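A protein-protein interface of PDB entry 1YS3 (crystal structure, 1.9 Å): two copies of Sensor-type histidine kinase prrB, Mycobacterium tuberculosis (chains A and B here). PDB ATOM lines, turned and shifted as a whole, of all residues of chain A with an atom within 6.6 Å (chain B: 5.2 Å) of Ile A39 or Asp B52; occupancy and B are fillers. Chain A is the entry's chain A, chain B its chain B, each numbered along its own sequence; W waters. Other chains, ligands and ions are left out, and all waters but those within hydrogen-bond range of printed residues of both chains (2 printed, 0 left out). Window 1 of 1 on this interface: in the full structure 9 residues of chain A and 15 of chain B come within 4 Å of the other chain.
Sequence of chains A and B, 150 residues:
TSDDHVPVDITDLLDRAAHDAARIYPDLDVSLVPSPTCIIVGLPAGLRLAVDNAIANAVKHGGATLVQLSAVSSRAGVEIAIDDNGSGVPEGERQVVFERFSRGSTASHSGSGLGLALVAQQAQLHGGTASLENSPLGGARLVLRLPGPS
NH1 of Arg B48 is in hydrogen-bond range of O of Thr A37 (3.4 Å). The side-chain hydroxyl (OG) of Ser A150 lies within hydrogen-bond range of the side-chain amide nitrogen (ND2) of Asn B53 (2.9 Å).
OD1 of Asp B52 is in salt-bridge range of NE of Arg B48, at 2.8 Å. The backbone carbonyl oxygen (O) of Asn B53 lies within hydrogen-bond range of the side-chain amide nitrogen (ND2) of Asn B57, at 2.9 Å. The side-chain carboxylate (OD1) of Asp A9 lies within hydrogen-bond range of the backbone NH (N) of Thr A11 (3.1 Å).
Among the printed residues, merely in contact across the chains: Pro A7 with Leu B49 (3.7 Å), Asp A9 with Ala B45 (3.9 Å), Ile A39 with Ala B45 (3.5 Å), Ile A39 with Arg B48 (3.4 Å), Ile A39 with Leu B49 (3.8 Å), Ile A39 with Asp B52 (3.8 Å), Val A41 with Leu B49 (3.8 Å), Pro A149 with Leu B49 (3.4 Å) and Ser A150 with Ala B56 (3.5 Å).
Ile A39 touches just these residues of chain B: Ala B45, Arg B48, Leu B49 and Asp B52. Of the printed residues of chain B, Pro A7 touches Leu B49. Of the printed residues of chain B, Thr A37 touches Arg B48. Of the printed residues of chain A, Asn B53 touches Ser A150. Of the printed residues of chain B, Val A41 touches Leu B49 (3.8 Å). Of the printed residues of chain B, Ser A150 touches Asn B53 (2.9 Å) and Ala B56 (3.5 Å). The nearest printed residue of chain B that does not touch Ser A150 is Asp B52 (4.3 Å).
Hydrophobic or aromatic side chains of chain A within 4 Å of the printed part of chain B: Pro A7, Ile A39, Val A41 and Pro A149. Of the 14 printed residues of chain B, 6 touch a printed residue of chain A. Hydrophobic or aromatic side chains of chain B within 4 Å of the printed part of chain A: Ala B45, Leu B49 and Ala B56. Along chain B the printed residues that touch a printed residue of chain A span positions 45 to 56. Among the printed residues, 11 pairs touch across the chains.
No position is printed for both chains. Of the 11 pairs that touch across the chains among the printed residues, none has its exchanged pair printed and touching as well.
Water W2 lies within hydrogen-bond range of the side-chain carboxylate (OD2) of Asp B52 (2.7 Å) and the backbone carbonyl oxygen (O) of Ile A39 (2.8 Å). Water W1 lies within hydrogen-bond range of the side-chain carboxylate of Asp B52 (2.7 Å), the backbone NH of Ile A39 (3.1 Å) and the guanidinium group of Arg B48 (3.4 Å).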
ATOM      1  N   VAL A   6      23.939  30.695   7.392  1.00  0.00           N
ATOM      2  CA  VAL A   6      23.452  30.857   8.756  1.00  0.00           C
ATOM      3  C   VAL A   6      23.144  29.470   9.305  1.00  0.00           C
ATOM      4  O   VAL A   6      23.113  28.493   8.564  1.00  0.00           O
ATOM      5  CB  VAL A   6      22.145  31.768   8.863  1.00  0.00           C
ATOM      6  CG1 VAL A   6      22.429  33.230   8.478  1.00  0.00           C
ATOM      7  CG2 VAL A   6      20.979  31.185   8.041  1.00  0.00           C
ATOM      8  N   PRO A   7      22.960  29.361  10.618  1.00  0.00           N
ATOM      9  CA  PRO A   7      22.586  28.074  11.236  1.00  0.00           C
ATOM     10  C   PRO A   7      21.227  27.625  10.703  1.00  0.00           C
ATOM     11  O   PRO A   7      20.295  28.440  10.634  1.00  0.00           O
ATOM     12  CB  PRO A   7      22.461  28.450  12.729  1.00  0.00           C
ATOM     13  CG  PRO A   7      23.458  29.591  12.881  1.00  0.00           C
ATOM     14  CD  PRO A   7      23.118  30.410  11.651  1.00  0.00           C
ATOM     15  N   VAL A   8      21.131  26.367  10.287  1.00  0.00           N
ATOM     16  CA  VAL A   8      19.890  25.859   9.728  1.00  0.00           C
ATOM     17  C   VAL A   8      19.617  24.575  10.462  1.00  0.00           C
ATOM     18  O   VAL A   8      20.441  23.682  10.446  1.00  0.00           O
ATOM     19  CB  VAL A   8      19.979  25.571   8.213  1.00  0.00           C
ATOM     20  CG1 VAL A   8      18.644  24.957   7.736  1.00  0.00           C
ATOM     21  CG2 VAL A   8      20.294  26.862   7.413  1.00  0.00           C
ATOM     22  N   ASP A   9      18.463  24.472  11.103  1.00  0.00           N
ATOM     23  CA  ASP A   9      18.041  23.195  11.693  1.00  0.00           C
ATOM     24  C   ASP A   9      17.398  22.388  10.550  1.00  0.00           C
ATOM     25  O   ASP A   9      16.238  22.609  10.153  1.00  0.00           O
ATOM     26  CB  ASP A   9      17.003  23.450  12.810  1.00  0.00           C
ATOM     27  CG  ASP A   9      16.441  22.165  13.386  1.00  0.00           C
ATOM     28  OD1 ASP A   9      16.591  21.091  12.739  1.00  0.00           O
ATOM     29  OD2 ASP A   9      15.841  22.220  14.486  1.00  0.00           O
ATOM     30  N   ILE A  10      18.193  21.498   9.981  1.00  0.00           N
ATOM     31  CA  ILE A  10      17.798  20.800   8.763  1.00  0.00           C
ATOM     32  C   ILE A  10      16.619  19.878   9.006  1.00  0.00           C
ATOM     33  O   ILE A  10      15.755  19.727   8.143  1.00  0.00           O
ATOM     34  CB  ILE A  10      19.026  20.087   8.094  1.00  0.00           C
ATOM     35  CG1 ILE A  10      18.684  19.659   6.654  1.00  0.00           C
ATOM     36  CG2 ILE A  10      19.435  18.941   8.841  1.00  0.00           C
ATOM     37  CD1 ILE A  10      18.559  20.897   5.660  1.00  0.00           C
ATOM     38  N   THR A  11      16.547  19.332  10.223  1.00  0.00           N
ATOM     39  CA  THR A  11      15.448  18.474  10.627  1.00  0.00           C
ATOM     40  C   THR A  11      14.103  19.242  10.638  1.00  0.00           C
ATOM     41  O   THR A  11      13.108  18.827  10.011  1.00  0.00           O
ATOM     42  CB  THR A  11      15.787  17.796  11.995  1.00  0.00           C
ATOM     43  OG1 THR A  11      17.058  17.144  11.873  1.00  0.00           O
ATOM     44  CG2 THR A  11      14.778  16.744  12.307  1.00  0.00           C
ATOM     45  N   THR A  37      17.424  16.033  15.719  1.00  0.00           N
ATOM     46  CA  THR A  37      17.758  17.387  15.338  1.00  0.00           C
ATOM     47  C   THR A  37      19.231  17.474  14.844  1.00  0.00           C
ATOM     48  O   THR A  37      20.147  16.863  15.440  1.00  0.00           O
ATOM     49  CB  THR A  37      17.397  18.281  16.520  1.00  0.00           C
ATOM     50  OG1 THR A  37      15.958  18.258  16.653  1.00  0.00           O
ATOM     51  CG2 THR A  37      17.833  19.727  16.299  1.00  0.00           C
ATOM     52  N   CYS A  38      19.424  18.137  13.699  1.00  0.00           N
ATOM     53  CA  CYS A  38      20.753  18.370  13.118  1.00  0.00           C
ATOM     54  C   CYS A  38      20.842  19.805  12.687  1.00  0.00           C
ATOM     55  O   CYS A  38      20.050  20.244  11.837  1.00  0.00           O
ATOM     56  CB  CYS A  38      21.008  17.488  11.890  1.00  0.00           C
ATOM     57  SG  CYS A  38      22.579  17.944  11.078  1.00  0.00           S
ATOM     58  N   ILE A  39      21.812  20.542  13.231  1.00  0.00           N
ATOM     59  CA  ILE A  39      22.084  21.889  12.725  1.00  0.00           C
ATOM     60  C   ILE A  39      23.297  21.924  11.753  1.00  0.00           C
ATOM     61  O   ILE A  39      24.388  21.445  12.107  1.00  0.00           O
ATOM     62  CB  ILE A  39      22.303  22.948  13.901  1.00  0.00           C
ATOM     63  CG1 ILE A  39      21.339  22.738  15.116  1.00  0.00           C
ATOM     64  CG2 ILE A  39      22.348  24.403  13.370  1.00  0.00           C
ATOM     65  CD1 ILE A  39      19.849  22.894  14.876  1.00  0.00           C
ATOM     66  N   ILE A  40      23.124  22.547  10.572  1.00  0.00           N
ATOM     67  CA  ILE A  40      24.274  22.849   9.763  1.00  0.00           C
ATOM     68  C   ILE A  40      24.344  24.332   9.579  1.00  0.00           C
ATOM     69  O   ILE A  40      23.488  25.098  10.053  1.00  0.00           O
ATOM     70  CB  ILE A  40      24.235  22.090   8.377  1.00  0.00           C
ATOM     71  CG1 ILE A  40      22.941  22.395   7.618  1.00  0.00           C
ATOM     72  CG2 ILE A  40      24.311  20.572   8.640  1.00  0.00           C
ATOM     73  CD1 ILE A  40      22.967  21.839   6.110  1.00  0.00           C
ATOM     74  N   VAL A  41      25.341  24.779   8.868  1.00  0.00           N
ATOM     75  CA  VAL A  41      25.391  26.193   8.521  1.00  0.00           C
ATOM     76  C   VAL A  41      25.176  26.135   7.014  1.00  0.00           C
ATOM     77  O   VAL A  41      25.790  25.287   6.337  1.00  0.00           O
ATOM     78  CB  VAL A  41      26.756  26.819   8.871  1.00  0.00           C
ATOM     79  CG1 VAL A  41      26.884  28.144   8.191  1.00  0.00           C
ATOM     80  CG2 VAL A  41      26.923  26.946  10.411  1.00  0.00           C
ATOM     81  N   GLY A 148      29.200  19.067   7.894  1.00  0.00           N
ATOM     82  CA  GLY A 148      28.753  19.553   9.188  1.00  0.00           C
ATOM     83  C   GLY A 148      29.590  20.785   9.544  1.00  0.00           C
ATOM     84  O   GLY A 148      30.640  21.047   8.922  1.00  0.00           O
ATOM     85  N   PRO A 149      29.103  21.584  10.506  1.00  0.00           N
ATOM     86  CA  PRO A 149      29.772  22.864  10.800  1.00  0.00           C
ATOM     87  C   PRO A 149      30.953  22.818  11.774  1.00  0.00           C
ATOM     88  O   PRO A 149      31.590  23.849  11.980  1.00  0.00           O
ATOM     89  CB  PRO A 149      28.627  23.700  11.387  1.00  0.00           C
ATOM     90  CG  PRO A 149      27.802  22.646  12.097  1.00  0.00           C
ATOM     91  CD  PRO A 149      27.817  21.448  11.227  1.00  0.00           C
ATOM     92  N   SER A 150      31.238  21.657  12.359  1.00  0.00           N
ATOM     93  CA  SER A 150      32.246  21.546  13.464  1.00  0.00           C
ATOM     94  C   SER A 150      33.562  20.842  13.085  1.00  0.00           C
ATOM     95  O   SER A 150      33.705  20.357  11.950  1.00  0.00           O
ATOM     96  CB  SER A 150      31.650  20.854  14.695  1.00  0.00           C
ATOM     97  OG  SER A 150      30.639  21.650  15.298  1.00  0.00           O
ATOM     98  OXT SER A 150      34.508  20.720  13.902  1.00  0.00           O
ATOM     99  N   ALA B  17      20.094  18.244  23.024  1.00  0.00           N
ATOM    100  CA  ALA B  17      21.480  18.313  22.578  1.00  0.00           C
ATOM    101  C   ALA B  17      22.319  17.183  23.187  1.00  0.00           C
ATOM    102  O   ALA B  17      23.163  16.595  22.528  1.00  0.00           O
ATOM    103  CB  ALA B  17      22.100  19.651  22.955  1.00  0.00           C
ATOM    104  N   TYR B  25      28.645  10.474  19.179  1.00  0.00           N
ATOM    105  CA  TYR B  25      29.939  10.132  19.725  1.00  0.00           C
ATOM    106  C   TYR B  25      29.724   8.919  20.644  1.00  0.00           C
ATOM    107  O   TYR B  25      29.196   9.048  21.771  1.00  0.00           O
ATOM    108  CB  TYR B  25      30.576  11.329  20.477  1.00  0.00           C
ATOM    109  CG  TYR B  25      30.545  12.646  19.709  1.00  0.00           C
ATOM    110  CD1 TYR B  25      31.583  13.008  18.836  1.00  0.00           C
ATOM    111  CD2 TYR B  25      29.484  13.539  19.879  1.00  0.00           C
ATOM    112  CE1 TYR B  25      31.542  14.226  18.140  1.00  0.00           C
ATOM    113  CE2 TYR B  25      29.436  14.730  19.196  1.00  0.00           C
ATOM    114  CZ  TYR B  25      30.454  15.068  18.327  1.00  0.00           C
ATOM    115  OH  TYR B  25      30.392  16.268  17.678  1.00  0.00           O
ATOM    116  N   PRO B  44      16.721  29.221  18.194  1.00  0.00           N
ATOM    117  CA  PRO B  44      16.968  27.858  18.645  1.00  0.00           C
ATOM    118  C   PRO B  44      18.019  27.117  17.789  1.00  0.00           C
ATOM    119  O   PRO B  44      18.764  26.302  18.341  1.00  0.00           O
ATOM    120  CB  PRO B  44      15.549  27.166  18.617  1.00  0.00           C
ATOM    121  CG  PRO B  44      14.648  28.058  18.057  1.00  0.00           C
ATOM    122  CD  PRO B  44      15.313  29.422  17.757  1.00  0.00           C
ATOM    123  N   ALA B  45      18.064  27.381  16.471  1.00  0.00           N
ATOM    124  CA  ALA B  45      19.077  26.691  15.578  1.00  0.00           C
ATOM    125  C   ALA B  45      20.482  27.163  15.984  1.00  0.00           C
ATOM    126  O   ALA B  45      21.386  26.365  16.166  1.00  0.00           O
ATOM    127  CB  ALA B  45      18.818  27.009  14.074  1.00  0.00           C
ATOM    128  N   ARG B  48      21.456  25.907  19.561  1.00  0.00           N
ATOM    129  CA  ARG B  48      21.781  24.495  19.543  1.00  0.00           C
ATOM    130  C   ARG B  48      23.140  24.251  18.870  1.00  0.00           C
ATOM    131  O   ARG B  48      23.961  23.480  19.357  1.00  0.00           O
ATOM    132  CB  ARG B  48      20.698  23.734  18.795  1.00  0.00           C
ATOM    133  CG  ARG B  48      21.138  22.316  18.445  1.00  0.00           C
ATOM    134  CD  ARG B  48      21.203  21.411  19.696  1.00  0.00           C
ATOM    135  NE  ARG B  48      21.602  20.094  19.186  1.00  0.00           N
ATOM    136  CZ  ARG B  48      20.812  19.042  19.028  1.00  0.00           C
ATOM    137  NH1 ARG B  48      21.327  17.954  18.485  1.00  0.00           N
ATOM    138  NH2 ARG B  48      19.553  19.051  19.425  1.00  0.00           N
ATOM    139  N   LEU B  49      23.368  24.927  17.766  1.00  0.00           N
ATOM    140  CA  LEU B  49      24.707  24.942  17.096  1.00  0.00           C
ATOM    141  C   LEU B  49      25.887  25.236  18.062  1.00  0.00           C
ATOM    142  O   LEU B  49      26.957  24.564  18.037  1.00  0.00           O
ATOM    143  CB  LEU B  49      24.686  25.951  15.940  1.00  0.00           C
ATOM    144  CG  LEU B  49      26.033  26.099  15.166  1.00  0.00           C
ATOM    145  CD1 LEU B  49      26.520  24.692  14.558  1.00  0.00           C
ATOM    146  CD2 LEU B  49      26.040  27.240  14.087  1.00  0.00           C
ATOM    147  N   ALA B  50      25.692  26.231  18.904  1.00  0.00           N
ATOM    148  CA  ALA B  50      26.738  26.708  19.808  1.00  0.00           C
ATOM    149  C   ALA B  50      27.065  25.549  20.746  1.00  0.00           C
ATOM    150  O   ALA B  50      28.249  25.180  20.929  1.00  0.00           O
ATOM    151  CB  ALA B  50      26.263  27.946  20.565  1.00  0.00           C
ATOM    152  N   VAL B  51      26.012  24.933  21.284  1.00  0.00           N
ATOM    153  CA  VAL B  51      26.173  23.724  22.123  1.00  0.00           C
ATOM    154  C   VAL B  51      26.861  22.587  21.346  1.00  0.00           C
ATOM    155  O   VAL B  51      27.790  21.964  21.888  1.00  0.00           O
ATOM    156  CB  VAL B  51      24.842  23.279  22.744  1.00  0.00           C
ATOM    157  CG1 VAL B  51      25.044  22.116  23.662  1.00  0.00           C
ATOM    158  CG2 VAL B  51      24.296  24.406  23.603  1.00  0.00           C
ATOM    159  N   ASP B  52      26.388  22.281  20.127  1.00  0.00           N
ATOM    160  CA  ASP B  52      26.943  21.183  19.349  1.00  0.00           C
ATOM    161  C   ASP B  52      28.395  21.461  19.149  1.00  0.00           C
ATOM    162  O   ASP B  52      29.214  20.555  19.199  1.00  0.00           O
ATOM    163  CB  ASP B  52      26.369  21.115  17.926  1.00  0.00           C
ATOM    164  CG  ASP B  52      24.909  20.767  17.882  1.00  0.00           C
ATOM    165  OD1 ASP B  52      24.346  20.223  18.864  1.00  0.00           O
ATOM    166  OD2 ASP B  52      24.333  21.043  16.796  1.00  0.00           O
ATOM    167  N   ASN B  53      28.723  22.718  18.826  1.00  0.00           N
ATOM    168  CA  ASN B  53      30.102  23.035  18.477  1.00  0.00           C
ATOM    169  C   ASN B  53      30.994  22.910  19.722  1.00  0.00           C
ATOM    170  O   ASN B  53      32.176  22.477  19.647  1.00  0.00           O
ATOM    171  CB  ASN B  53      30.167  24.433  17.819  1.00  0.00           C
ATOM    172  CG  ASN B  53      31.565  24.788  17.289  1.00  0.00           C
ATOM    173  OD1 ASN B  53      32.153  25.778  17.719  1.00  0.00           O
ATOM    174  ND2 ASN B  53      32.089  23.983  16.358  1.00  0.00           N
ATOM    175  N   ALA B  54      30.454  23.296  20.880  1.00  0.00           N
ATOM    176  CA  ALA B  54      31.198  23.154  22.150  1.00  0.00           C
ATOM    177  C   ALA B  54      31.512  21.667  22.451  1.00  0.00           C
ATOM    178  O   ALA B  54      32.667  21.298  22.766  1.00  0.00           O
ATOM    179  CB  ALA B  54      30.433  23.829  23.288  1.00  0.00           C
ATOM    180  N   ILE B  55      30.519  20.805  22.313  1.00  0.00           N
ATOM    181  CA  ILE B  55      30.703  19.352  22.500  1.00  0.00           C
ATOM    182  C   ILE B  55      31.666  18.788  21.438  1.00  0.00           C
ATOM    183  O   ILE B  55      32.539  17.973  21.743  1.00  0.00           O
ATOM    184  CB  ILE B  55      29.333  18.612  22.432  1.00  0.00           C
ATOM    185  CG1 ILE B  55      28.401  19.134  23.540  1.00  0.00           C
ATOM    186  CG2 ILE B  55      29.504  17.095  22.501  1.00  0.00           C
ATOM    187  CD1 ILE B  55      26.856  18.665  23.405  1.00  0.00           C
ATOM    188  N   ALA B  56      31.542  19.247  20.199  1.00  0.00           N
ATOM    189  CA  ALA B  56      32.386  18.737  19.135  1.00  0.00           C
ATOM    190  C   ALA B  56      33.836  19.079  19.436  1.00  0.00           C
ATOM    191  O   ALA B  56      34.710  18.257  19.256  1.00  0.00           O
ATOM    192  CB  ALA B  56      31.984  19.298  17.776  1.00  0.00           C
ATOM    193  N   ASN B  57      34.100  20.295  19.883  1.00  0.00           N
ATOM    194  CA  ASN B  57      35.467  20.670  20.232  1.00  0.00           C
ATOM    195  C   ASN B  57      36.023  19.879  21.421  1.00  0.00           C
ATOM    196  O   ASN B  57      37.206  19.466  21.406  1.00  0.00           O
ATOM    197  CB  ASN B  57      35.571  22.155  20.467  1.00  0.00           C
ATOM    198  CG  ASN B  57      35.791  22.911  19.191  1.00  0.00           C
ATOM    199  OD1 ASN B  57      36.921  23.253  18.852  1.00  0.00           O
ATOM    200  ND2 ASN B  57      34.726  23.129  18.444  1.00  0.00           N
HETATM  201  O   HOH W   1      22.932  19.031  15.640  1.00  0.00           O
HETATM  202  O   HOH W   2      25.728  20.902  14.480  1.00  0.00           O
